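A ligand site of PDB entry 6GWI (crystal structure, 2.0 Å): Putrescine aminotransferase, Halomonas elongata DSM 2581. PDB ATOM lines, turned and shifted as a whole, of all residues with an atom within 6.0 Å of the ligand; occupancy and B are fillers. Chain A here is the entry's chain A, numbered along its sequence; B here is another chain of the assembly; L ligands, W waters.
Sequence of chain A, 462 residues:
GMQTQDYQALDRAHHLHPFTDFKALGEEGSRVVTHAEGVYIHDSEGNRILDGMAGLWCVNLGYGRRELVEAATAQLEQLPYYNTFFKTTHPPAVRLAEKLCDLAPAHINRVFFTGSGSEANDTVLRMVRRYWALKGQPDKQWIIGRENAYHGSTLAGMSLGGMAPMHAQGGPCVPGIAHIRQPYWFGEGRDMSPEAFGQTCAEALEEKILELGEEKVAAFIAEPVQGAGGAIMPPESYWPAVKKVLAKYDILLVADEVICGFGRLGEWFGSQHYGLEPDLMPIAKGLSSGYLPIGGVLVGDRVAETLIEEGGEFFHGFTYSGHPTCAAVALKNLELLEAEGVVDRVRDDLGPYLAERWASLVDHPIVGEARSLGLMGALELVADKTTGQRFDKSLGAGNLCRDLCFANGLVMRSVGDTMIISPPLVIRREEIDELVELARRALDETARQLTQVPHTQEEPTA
The side-chain hydroxyl (OG) of Ser 118 is in hydrogen-bond range of an oxygen (O4) of the ligand, at 2.6 Å.
An oxygen (O3) of the ligand sits at hydrogen-bond distance from the side-chain hydroxyl (OG1) of Thr 319 of chain B, 2.7 Å away.
The side-chain amino group (NZ) of Lys 285 is bonded to a carbon (C5) of the ligand (1.4 Å).
N of Gly 117 sits at hydrogen-bond distance from O5 of the ligand (2.9 Å).
An oxygen (O3) of the ligand lies within hydrogen-bond range of the backbone NH of Thr 319 of chain B (2.8 Å).
A nitrogen (N1) of the ligand is in hydrogen-bond range of the side-chain carboxylate (OD2) of Asp 256.
An oxygen (O4) of the ligand sits at hydrogen-bond distance from the backbone NH (N) of Ser 118, at 2.7 Å.
ND2 of Asn 121 sits at hydrogen-bond distance from O of His 151 (2.9 Å).
OH of Tyr 320 of chain B sits at hydrogen-bond distance from O of Lys 285.
OG of Ser 118 lies within hydrogen-bond range of N of Ser 153 (2.8 Å).
The side-chain amide nitrogen of Asn 121 lies within hydrogen-bond range of the backbone carbonyl oxygen of Gly 117, at 3.2 Å.
OD1 of Asp 256 sits at hydrogen-bond distance from N of Val 258, at 3.1 Å.
The side-chain amino group (NZ) of Lys 285 lies close to the side-chain hydroxyl (OG1) of Thr 319 of chain B (3.4 Å).
The side-chain carboxylate (OD2) of Asp 256 sits at hydrogen-bond distance from the side-chain amide nitrogen (ND2) of Asn 121.
The side-chain carboxylate of Glu 223 is in hydrogen-bond range of the backbone NH of Tyr 150, 3.0 Å away.
O of Tyr 150 sits close to N1 of the ligand (3.5 Å).
CB of Ser 116 touches O4 of the ligand (3.5 Å).
Asn 121 touches the ligand.
C of His 151 touches C7 of the ligand (3.5 Å).
Gly 152 touches the ligand (CA to C8, 3.5 Å).
Glu 223 touches the ligand (OE1 to C2, 3.5 Å).
CB of Val 258 touches C1 of the ligand, 3.6 Å away.
CD1 of Ile 259 touches O1 of the ligand, at 3.1 Å.
Phe 318 of chain B touches the ligand.
Hydrophobic or aromatic side chains that line the ligand: Tyr 150, Val 258, Ile 259 and Phe 318 of chain B.
Within 4 Å of the ligand: Ser 116, Gly 117, Ser 118, Asn 121, Tyr 150, His 151, Gly 152, Glu 223, Asp 256, Val 258, Ile 259, Lys 285, Phe 318 of chain B and Thr 319 of chain B.
Along chain A the residues within 4 Å of the ligand span positions 116 to 285.
The nearest printed residue that does not touch the ligand is Ala 284 (4.5 Å).
Water W1 lies within hydrogen-bond range of O5 of the ligand (2.6 Å), N of Tyr 320 of chain B (2.8 Å) and N of Thr 319 of chain B (3.4 Å).
Water W2 bridges an oxygen (O5) of the ligand (2.7 Å) and the backbone NH (N) of Lys 285 (3.2 Å).
Water W3 lies within hydrogen-bond range of OE1 of Glu 223 (2.8 Å), O1 of the ligand (2.8 Å) and N of Ala 228 (2.8 Å).
Water W4 lies within hydrogen-bond range of the side-chain hydroxyl (OH) of Tyr 150 (2.6 Å), the backbone carbonyl oxygen (O) of Gly 317 of chain B (2.8 Å) and an oxygen (O3) of the ligand (2.9 Å).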
ATOM      1  N   TRP A  57      13.178  11.306   6.018  1.00  0.00           N
ATOM      2  CA  TRP A  57      13.052  12.697   6.444  1.00  0.00           C
ATOM      3  C   TRP A  57      12.312  12.845   7.765  1.00  0.00           C
ATOM      4  O   TRP A  57      11.766  13.917   8.040  1.00  0.00           O
ATOM      5  CB  TRP A  57      12.318  13.590   5.426  1.00  0.00           C
ATOM      6  CG  TRP A  57      12.616  13.490   3.974  1.00  0.00           C
ATOM      7  CD1 TRP A  57      12.146  12.559   3.103  1.00  0.00           C
ATOM      8  CD2 TRP A  57      13.385  14.420   3.187  1.00  0.00           C
ATOM      9  NE1 TRP A  57      12.587  12.831   1.822  1.00  0.00           N
ATOM     10  CE2 TRP A  57      13.349  13.970   1.860  1.00  0.00           C
ATOM     11  CE3 TRP A  57      14.098  15.586   3.485  1.00  0.00           C
ATOM     12  CZ2 TRP A  57      14.012  14.635   0.822  1.00  0.00           C
ATOM     13  CZ3 TRP A  57      14.757  16.247   2.455  1.00  0.00           C
ATOM     14  CH2 TRP A  57      14.704  15.769   1.142  1.00  0.00           C
ATOM     15  N   GLY A 115      -3.570   9.957   9.248  1.00  0.00           N
ATOM     16  CA  GLY A 115      -2.549   8.953   9.455  1.00  0.00           C
ATOM     17  C   GLY A 115      -1.257   9.224   8.712  1.00  0.00           C
ATOM     18  O   GLY A 115      -0.203   8.674   9.064  1.00  0.00           O
ATOM     19  N   SER A 116      -1.302  10.090   7.695  1.00  0.00           N
ATOM     20  CA  SER A 116      -0.179  10.268   6.795  1.00  0.00           C
ATOM     21  C   SER A 116      -0.182  11.682   6.236  1.00  0.00           C
ATOM     22  O   SER A 116      -1.178  12.402   6.300  1.00  0.00           O
ATOM     23  CB  SER A 116      -0.242   9.262   5.642  1.00  0.00           C
ATOM     24  OG  SER A 116      -1.411   9.467   4.871  1.00  0.00           O
ATOM     25  N   GLY A 117       0.956  12.061   5.639  1.00  0.00           N
ATOM     26  CA  GLY A 117       1.016  13.316   4.918  1.00  0.00           C
ATOM     27  C   GLY A 117       0.162  13.303   3.680  1.00  0.00           C
ATOM     28  O   GLY A 117      -0.381  14.340   3.273  1.00  0.00           O
ATOM     29  N   SER A 118       0.011  12.135   3.041  1.00  0.00           N
ATOM     30  CA  SER A 118      -0.873  12.037   1.884  1.00  0.00           C
ATOM     31  C   SER A 118      -2.316  12.311   2.275  1.00  0.00           C
ATOM     32  O   SER A 118      -2.995  13.137   1.650  1.00  0.00           O
ATOM     33  CB  SER A 118      -0.736  10.653   1.229  1.00  0.00           C
ATOM     34  OG  SER A 118       0.517  10.483   0.595  1.00  0.00           O
ATOM     35  N   GLU A 119      -2.811  11.623   3.302  1.00  0.00           N
ATOM     36  CA  GLU A 119      -4.176  11.858   3.773  1.00  0.00           C
ATOM     37  C   GLU A 119      -4.373  13.292   4.239  1.00  0.00           C
ATOM     38  O   GLU A 119      -5.471  13.829   4.132  1.00  0.00           O
ATOM     39  CB  GLU A 119      -4.526  10.901   4.913  1.00  0.00           C
ATOM     40  CG  GLU A 119      -4.668   9.433   4.491  1.00  0.00           C
ATOM     41  CD  GLU A 119      -4.942   8.516   5.669  1.00  0.00           C
ATOM     42  OE1 GLU A 119      -5.222   7.319   5.430  1.00  0.00           O
ATOM     43  OE2 GLU A 119      -4.853   8.969   6.829  1.00  0.00           O
ATOM     44  N   ASN A 121      -3.018  15.919   2.841  1.00  0.00           N
ATOM     45  CA  ASN A 121      -3.254  16.730   1.644  1.00  0.00           C
ATOM     46  C   ASN A 121      -4.619  16.456   1.021  1.00  0.00           C
ATOM     47  O   ASN A 121      -5.208  17.365   0.413  1.00  0.00           O
ATOM     48  CB  ASN A 121      -2.117  16.517   0.644  1.00  0.00           C
ATOM     49  CG  ASN A 121      -0.907  17.392   0.940  1.00  0.00           C
ATOM     50  OD1 ASN A 121      -1.009  18.617   0.925  1.00  0.00           O
ATOM     51  ND2 ASN A 121       0.221  16.775   1.255  1.00  0.00           N
ATOM     52  N   TYR A 150       6.012  17.677  -4.408  1.00  0.00           N
ATOM     53  CA  TYR A 150       5.551  16.392  -3.891  1.00  0.00           C
ATOM     54  C   TYR A 150       4.581  16.647  -2.746  1.00  0.00           C
ATOM     55  O   TYR A 150       4.945  17.260  -1.748  1.00  0.00           O
ATOM     56  CB  TYR A 150       6.708  15.513  -3.431  1.00  0.00           C
ATOM     57  CG  TYR A 150       6.241  14.103  -3.128  1.00  0.00           C
ATOM     58  CD1 TYR A 150       6.127  13.155  -4.145  1.00  0.00           C
ATOM     59  CD2 TYR A 150       5.857  13.734  -1.846  1.00  0.00           C
ATOM     60  CE1 TYR A 150       5.686  11.876  -3.878  1.00  0.00           C
ATOM     61  CE2 TYR A 150       5.418  12.463  -1.575  1.00  0.00           C
ATOM     62  CZ  TYR A 150       5.324  11.537  -2.594  1.00  0.00           C
ATOM     63  OH  TYR A 150       4.879  10.254  -2.319  1.00  0.00           O
ATOM     64  N   HIS A 151       3.356  16.143  -2.902  1.00  0.00           N
ATOM     65  CA  HIS A 151       2.310  16.323  -1.901  1.00  0.00           C
ATOM     66  C   HIS A 151       1.651  15.002  -1.533  1.00  0.00           C
ATOM     67  O   HIS A 151       0.518  14.999  -1.047  1.00  0.00           O
ATOM     68  CB  HIS A 151       1.283  17.343  -2.393  1.00  0.00           C
ATOM     69  CG  HIS A 151       1.858  18.701  -2.643  1.00  0.00           C
ATOM     70  ND1 HIS A 151       2.381  19.470  -1.627  1.00  0.00           N
ATOM     71  CD2 HIS A 151       1.987  19.426  -3.773  1.00  0.00           C
ATOM     72  CE1 HIS A 151       2.824  20.614  -2.132  1.00  0.00           C
ATOM     73  NE2 HIS A 151       2.586  20.615  -3.432  1.00  0.00           N
ATOM     74  N   GLY A 152       2.321  13.875  -1.772  1.00  0.00           N
ATOM     75  CA  GLY A 152       1.841  12.583  -1.346  1.00  0.00           C
ATOM     76  C   GLY A 152       1.501  11.683  -2.514  1.00  0.00           C
ATOM     77  O   GLY A 152       1.761  11.979  -3.678  1.00  0.00           O
ATOM     78  N   SER A 153       0.886  10.537  -2.164  1.00  0.00           N
ATOM     79  CA  SER A 153       0.721   9.440  -3.105  1.00  0.00           C
ATOM     80  C   SER A 153      -0.699   8.910  -3.153  1.00  0.00           C
ATOM     81  O   SER A 153      -0.936   7.871  -3.783  1.00  0.00           O
ATOM     82  CB  SER A 153       1.685   8.303  -2.743  1.00  0.00           C
ATOM     83  OG  SER A 153       1.743   7.335  -3.779  1.00  0.00           O
ATOM     84  N   GLU A 223       5.528  23.460  -0.791  1.00  0.00           N
ATOM     85  CA  GLU A 223       6.485  23.171   0.267  1.00  0.00           C
ATOM     86  C   GLU A 223       7.352  24.403   0.474  1.00  0.00           C
ATOM     87  O   GLU A 223       7.869  24.950  -0.506  1.00  0.00           O
ATOM     88  CB  GLU A 223       7.359  21.976  -0.120  1.00  0.00           C
ATOM     89  CG  GLU A 223       6.603  20.714  -0.550  1.00  0.00           C
ATOM     90  CD  GLU A 223       7.474  19.760  -1.367  1.00  0.00           C
ATOM     91  OE1 GLU A 223       8.378  19.121  -0.795  1.00  0.00           O
ATOM     92  OE2 GLU A 223       7.269  19.676  -2.599  1.00  0.00           O
ATOM     93  N   GLY A 227      11.295  18.997  -0.907  1.00  0.00           N
ATOM     94  CA  GLY A 227      12.060  17.879  -0.392  1.00  0.00           C
ATOM     95  C   GLY A 227      12.313  16.782  -1.396  1.00  0.00           C
ATOM     96  O   GLY A 227      13.412  16.684  -1.963  1.00  0.00           O
ATOM     97  N   ALA A 228      11.297  15.957  -1.653  1.00  0.00           N
ATOM     98  CA  ALA A 228      11.471  14.827  -2.556  1.00  0.00           C
ATOM     99  C   ALA A 228      11.942  15.269  -3.928  1.00  0.00           C
ATOM    100  O   ALA A 228      12.630  14.500  -4.628  1.00  0.00           O
ATOM    101  CB  ALA A 228      10.151  14.055  -2.682  1.00  0.00           C
ATOM    102  N   ASP A 256       2.817  23.139   2.785  1.00  0.00           N
ATOM    103  CA  ASP A 256       2.973  21.712   3.040  1.00  0.00           C
ATOM    104  C   ASP A 256       4.225  21.513   3.890  1.00  0.00           C
ATOM    105  O   ASP A 256       5.352  21.599   3.376  1.00  0.00           O
ATOM    106  CB  ASP A 256       3.051  20.920   1.734  1.00  0.00           C
ATOM    107  CG  ASP A 256       3.055  19.411   1.960  1.00  0.00           C
ATOM    108  OD1 ASP A 256       3.430  18.962   3.070  1.00  0.00           O
ATOM    109  OD2 ASP A 256       2.674  18.671   1.031  1.00  0.00           O
ATOM    110  N   GLU A 257       4.019  21.220   5.164  1.00  0.00           N
ATOM    111  CA  GLU A 257       5.093  21.157   6.158  1.00  0.00           C
ATOM    112  C   GLU A 257       5.483  19.726   6.502  1.00  0.00           C
ATOM    113  O   GLU A 257       6.145  19.499   7.524  1.00  0.00           O
ATOM    114  CB  GLU A 257       4.644  21.884   7.424  1.00  0.00           C
ATOM    115  CG  GLU A 257       4.397  23.381   7.248  1.00  0.00           C
ATOM    116  CD  GLU A 257       5.667  24.212   7.296  1.00  0.00           C
ATOM    117  OE1 GLU A 257       5.579  25.447   7.130  1.00  0.00           O
ATOM    118  OE2 GLU A 257       6.753  23.634   7.503  1.00  0.00           O
ATOM    119  N   VAL A 258       5.116  18.751   5.672  1.00  0.00           N
ATOM    120  CA  VAL A 258       5.330  17.355   6.028  1.00  0.00           C
ATOM    121  C   VAL A 258       6.809  17.063   6.240  1.00  0.00           C
ATOM    122  O   VAL A 258       7.181  16.335   7.168  1.00  0.00           O
ATOM    123  CB  VAL A 258       4.700  16.425   4.972  1.00  0.00           C
ATOM    124  CG1 VAL A 258       5.133  14.980   5.184  1.00  0.00           C
ATOM    125  CG2 VAL A 258       3.174  16.531   5.034  1.00  0.00           C
ATOM    126  N   ILE A 259       7.671  17.633   5.404  1.00  0.00           N
ATOM    127  CA  ILE A 259       9.118  17.516   5.592  1.00  0.00           C
ATOM    128  C   ILE A 259       9.664  18.671   6.413  1.00  0.00           C
ATOM    129  O   ILE A 259      10.498  18.465   7.296  1.00  0.00           O
ATOM    130  CB  ILE A 259       9.844  17.413   4.232  1.00  0.00           C
ATOM    131  CG1 ILE A 259       9.811  15.974   3.714  1.00  0.00           C
ATOM    132  CG2 ILE A 259      11.282  17.934   4.336  1.00  0.00           C
ATOM    133  CD1 ILE A 259      10.431  15.792   2.353  1.00  0.00           C
ATOM    134  N   ALA A 284       3.217  15.606   9.067  1.00  0.00           N
ATOM    135  CA  ALA A 284       3.396  14.184   9.351  1.00  0.00           C
ATOM    136  C   ALA A 284       4.864  13.952   9.686  1.00  0.00           C
ATOM    137  O   ALA A 284       5.486  14.794  10.355  1.00  0.00           O
ATOM    138  CB  ALA A 284       2.956  13.320   8.177  1.00  0.00           C
ATOM    139  N   LYS A 285       5.424  12.814   9.276  1.00  0.00           N
ATOM    140  CA  LYS A 285       6.843  12.523   9.391  1.00  0.00           C
ATOM    141  C   LYS A 285       7.413  12.907  10.757  1.00  0.00           C
ATOM    142  O   LYS A 285       7.231  12.158  11.730  1.00  0.00           O
ATOM    143  CB  LYS A 285       7.608  13.228   8.257  1.00  0.00           C
ATOM    144  CG  LYS A 285       7.392  12.551   6.903  1.00  0.00           C
ATOM    145  CD  LYS A 285       8.294  13.098   5.803  1.00  0.00           C
ATOM    146  CE  LYS A 285       8.153  12.269   4.524  1.00  0.00           C
ATOM    147  NZ  LYS A 285       7.056  12.720   3.597  1.00  0.00           N
ATOM    148  N   PHE B  85      11.264   2.129   0.874  1.00  0.00           N
ATOM    149  CA  PHE B  85      11.517   2.801  -0.395  1.00  0.00           C
ATOM    150  C   PHE B  85      12.894   2.472  -0.990  1.00  0.00           C
ATOM    151  O   PHE B  85      13.022   2.312  -2.209  1.00  0.00           O
ATOM    152  CB  PHE B  85      11.447   4.324  -0.226  1.00  0.00           C
ATOM    153  CG  PHE B  85      10.057   4.876  -0.024  1.00  0.00           C
ATOM    154  CD1 PHE B  85       9.564   5.873  -0.860  1.00  0.00           C
ATOM    155  CD2 PHE B  85       9.240   4.423   1.008  1.00  0.00           C
ATOM    156  CE1 PHE B  85       8.288   6.400  -0.677  1.00  0.00           C
ATOM    157  CE2 PHE B  85       7.973   4.947   1.194  1.00  0.00           C
ATOM    158  CZ  PHE B  85       7.493   5.937   0.351  1.00  0.00           C
ATOM    159  N   GLU B 119      -6.233   4.889   2.032  1.00  0.00           N
ATOM    160  CA  GLU B 119      -5.049   4.815   1.189  1.00  0.00           C
ATOM    161  C   GLU B 119      -5.000   3.498   0.424  1.00  0.00           C
ATOM    162  O   GLU B 119      -4.477   3.447  -0.694  1.00  0.00           O
ATOM    163  CB  GLU B 119      -3.785   4.955   2.041  1.00  0.00           C
ATOM    164  CG  GLU B 119      -3.559   6.349   2.605  1.00  0.00           C
ATOM    165  CD  GLU B 119      -2.358   6.401   3.529  1.00  0.00           C
ATOM    166  OE1 GLU B 119      -1.944   7.524   3.902  1.00  0.00           O
ATOM    167  OE2 GLU B 119      -1.819   5.332   3.868  1.00  0.00           O
ATOM    168  N   GLY B 317       3.214   5.049  -3.198  1.00  0.00           N
ATOM    169  CA  GLY B 317       3.472   4.524  -1.880  1.00  0.00           C
ATOM    170  C   GLY B 317       3.533   5.614  -0.840  1.00  0.00           C
ATOM    171  O   GLY B 317       3.497   6.809  -1.132  1.00  0.00           O
ATOM    172  N   PHE B 318       3.620   5.184   0.419  1.00  0.00           N
ATOM    173  CA  PHE B 318       3.523   6.077   1.560  1.00  0.00           C
ATOM    174  C   PHE B 318       4.681   5.877   2.516  1.00  0.00           C
ATOM    175  O   PHE B 318       5.160   4.761   2.722  1.00  0.00           O
ATOM    176  CB  PHE B 318       2.187   5.854   2.286  1.00  0.00           C
ATOM    177  CG  PHE B 318       0.995   5.893   1.360  1.00  0.00           C
ATOM    178  CD1 PHE B 318       0.393   7.098   1.034  1.00  0.00           C
ATOM    179  CD2 PHE B 318       0.508   4.736   0.788  1.00  0.00           C
ATOM    180  CE1 PHE B 318      -0.691   7.137   0.173  1.00  0.00           C
ATOM    181  CE2 PHE B 318      -0.567   4.763  -0.074  1.00  0.00           C
ATOM    182  CZ  PHE B 318      -1.169   5.966  -0.375  1.00  0.00           C
ATOM    183  N   THR B 319       5.137   6.996   3.102  1.00  0.00           N
ATOM    184  CA  THR B 319       6.229   6.990   4.072  1.00  0.00           C
ATOM    185  C   THR B 319       6.077   5.867   5.077  1.00  0.00           C
ATOM    186  O   THR B 319       7.047   5.154   5.389  1.00  0.00           O
ATOM    187  CB  THR B 319       6.287   8.347   4.781  1.00  0.00           C
ATOM    188  OG1 THR B 319       6.580   9.389   3.836  1.00  0.00           O
ATOM    189  CG2 THR B 319       7.338   8.356   5.858  1.00  0.00           C
ATOM    190  N   TYR B 320       4.867   5.667   5.587  1.00  0.00           N
ATOM    191  CA  TYR B 320       4.617   4.680   6.634  1.00  0.00           C
ATOM    192  C   TYR B 320       4.092   3.360   6.076  1.00  0.00           C
ATOM    193  O   TYR B 320       3.602   2.522   6.848  1.00  0.00           O
ATOM    194  CB  TYR B 320       3.652   5.269   7.663  1.00  0.00           C
ATOM    195  CG  TYR B 320       4.238   6.464   8.401  1.00  0.00           C
ATOM    196  CD1 TYR B 320       5.557   6.441   8.845  1.00  0.00           C
ATOM    197  CD2 TYR B 320       3.488   7.607   8.648  1.00  0.00           C
ATOM    198  CE1 TYR B 320       6.117   7.512   9.521  1.00  0.00           C
ATOM    199  CE2 TYR B 320       4.041   8.698   9.330  1.00  0.00           C
ATOM    200  CZ  TYR B 320       5.351   8.636   9.763  1.00  0.00           C
ATOM    201  OH  TYR B 320       5.910   9.699  10.435  1.00  0.00           O
HETATM  202  N1  LIG L   1       3.971  16.191   1.391  1.00  0.00           N
HETATM  203  C1  LIG L   1       5.344  16.260   1.395  1.00  0.00           C
HETATM  204  C2  LIG L   1       6.012  17.598   1.230  1.00  0.00           C
HETATM  205  C3  LIG L   1       6.096  15.090   1.563  1.00  0.00           C
HETATM  206  O1  LIG L   1       7.471  15.176   1.577  1.00  0.00           O
HETATM  207  C4  LIG L   1       5.466  13.862   1.728  1.00  0.00           C
HETATM  208  C5  LIG L   1       6.206  12.740   2.427  1.00  0.00           C
HETATM  209  C6  LIG L   1       4.072  13.815   1.709  1.00  0.00           C
HETATM  210  C7  LIG L   1       3.328  14.974   1.540  1.00  0.00           C
HETATM  211  C8  LIG L   1       3.335  12.499   1.868  1.00  0.00           C
HETATM  212  O2  LIG L   1       3.372  12.014   3.198  1.00  0.00           O
HETATM  213  P1  LIG L   1       3.074  10.457   3.445  1.00  0.00           P
HETATM  214  O3  LIG L   1       4.150   9.645   2.769  1.00  0.00           O
HETATM  215  O4  LIG L   1       1.716  10.108   2.853  1.00  0.00           O
HETATM  216  O5  LIG L   1       3.080  10.187   4.933  1.00  0.00           O
HETATM  217  O   HOH W   1       2.830   7.638   5.473  1.00  0.00           O
HETATM  218  O   HOH W   2       4.610  10.658   7.120  1.00  0.00           O
HETATM  219  O   HOH W   3       8.733  16.369  -0.614  1.00  0.00           O
HETATM  220  O   HOH W   4       3.878   9.379  -0.137  1.00  0.00           O
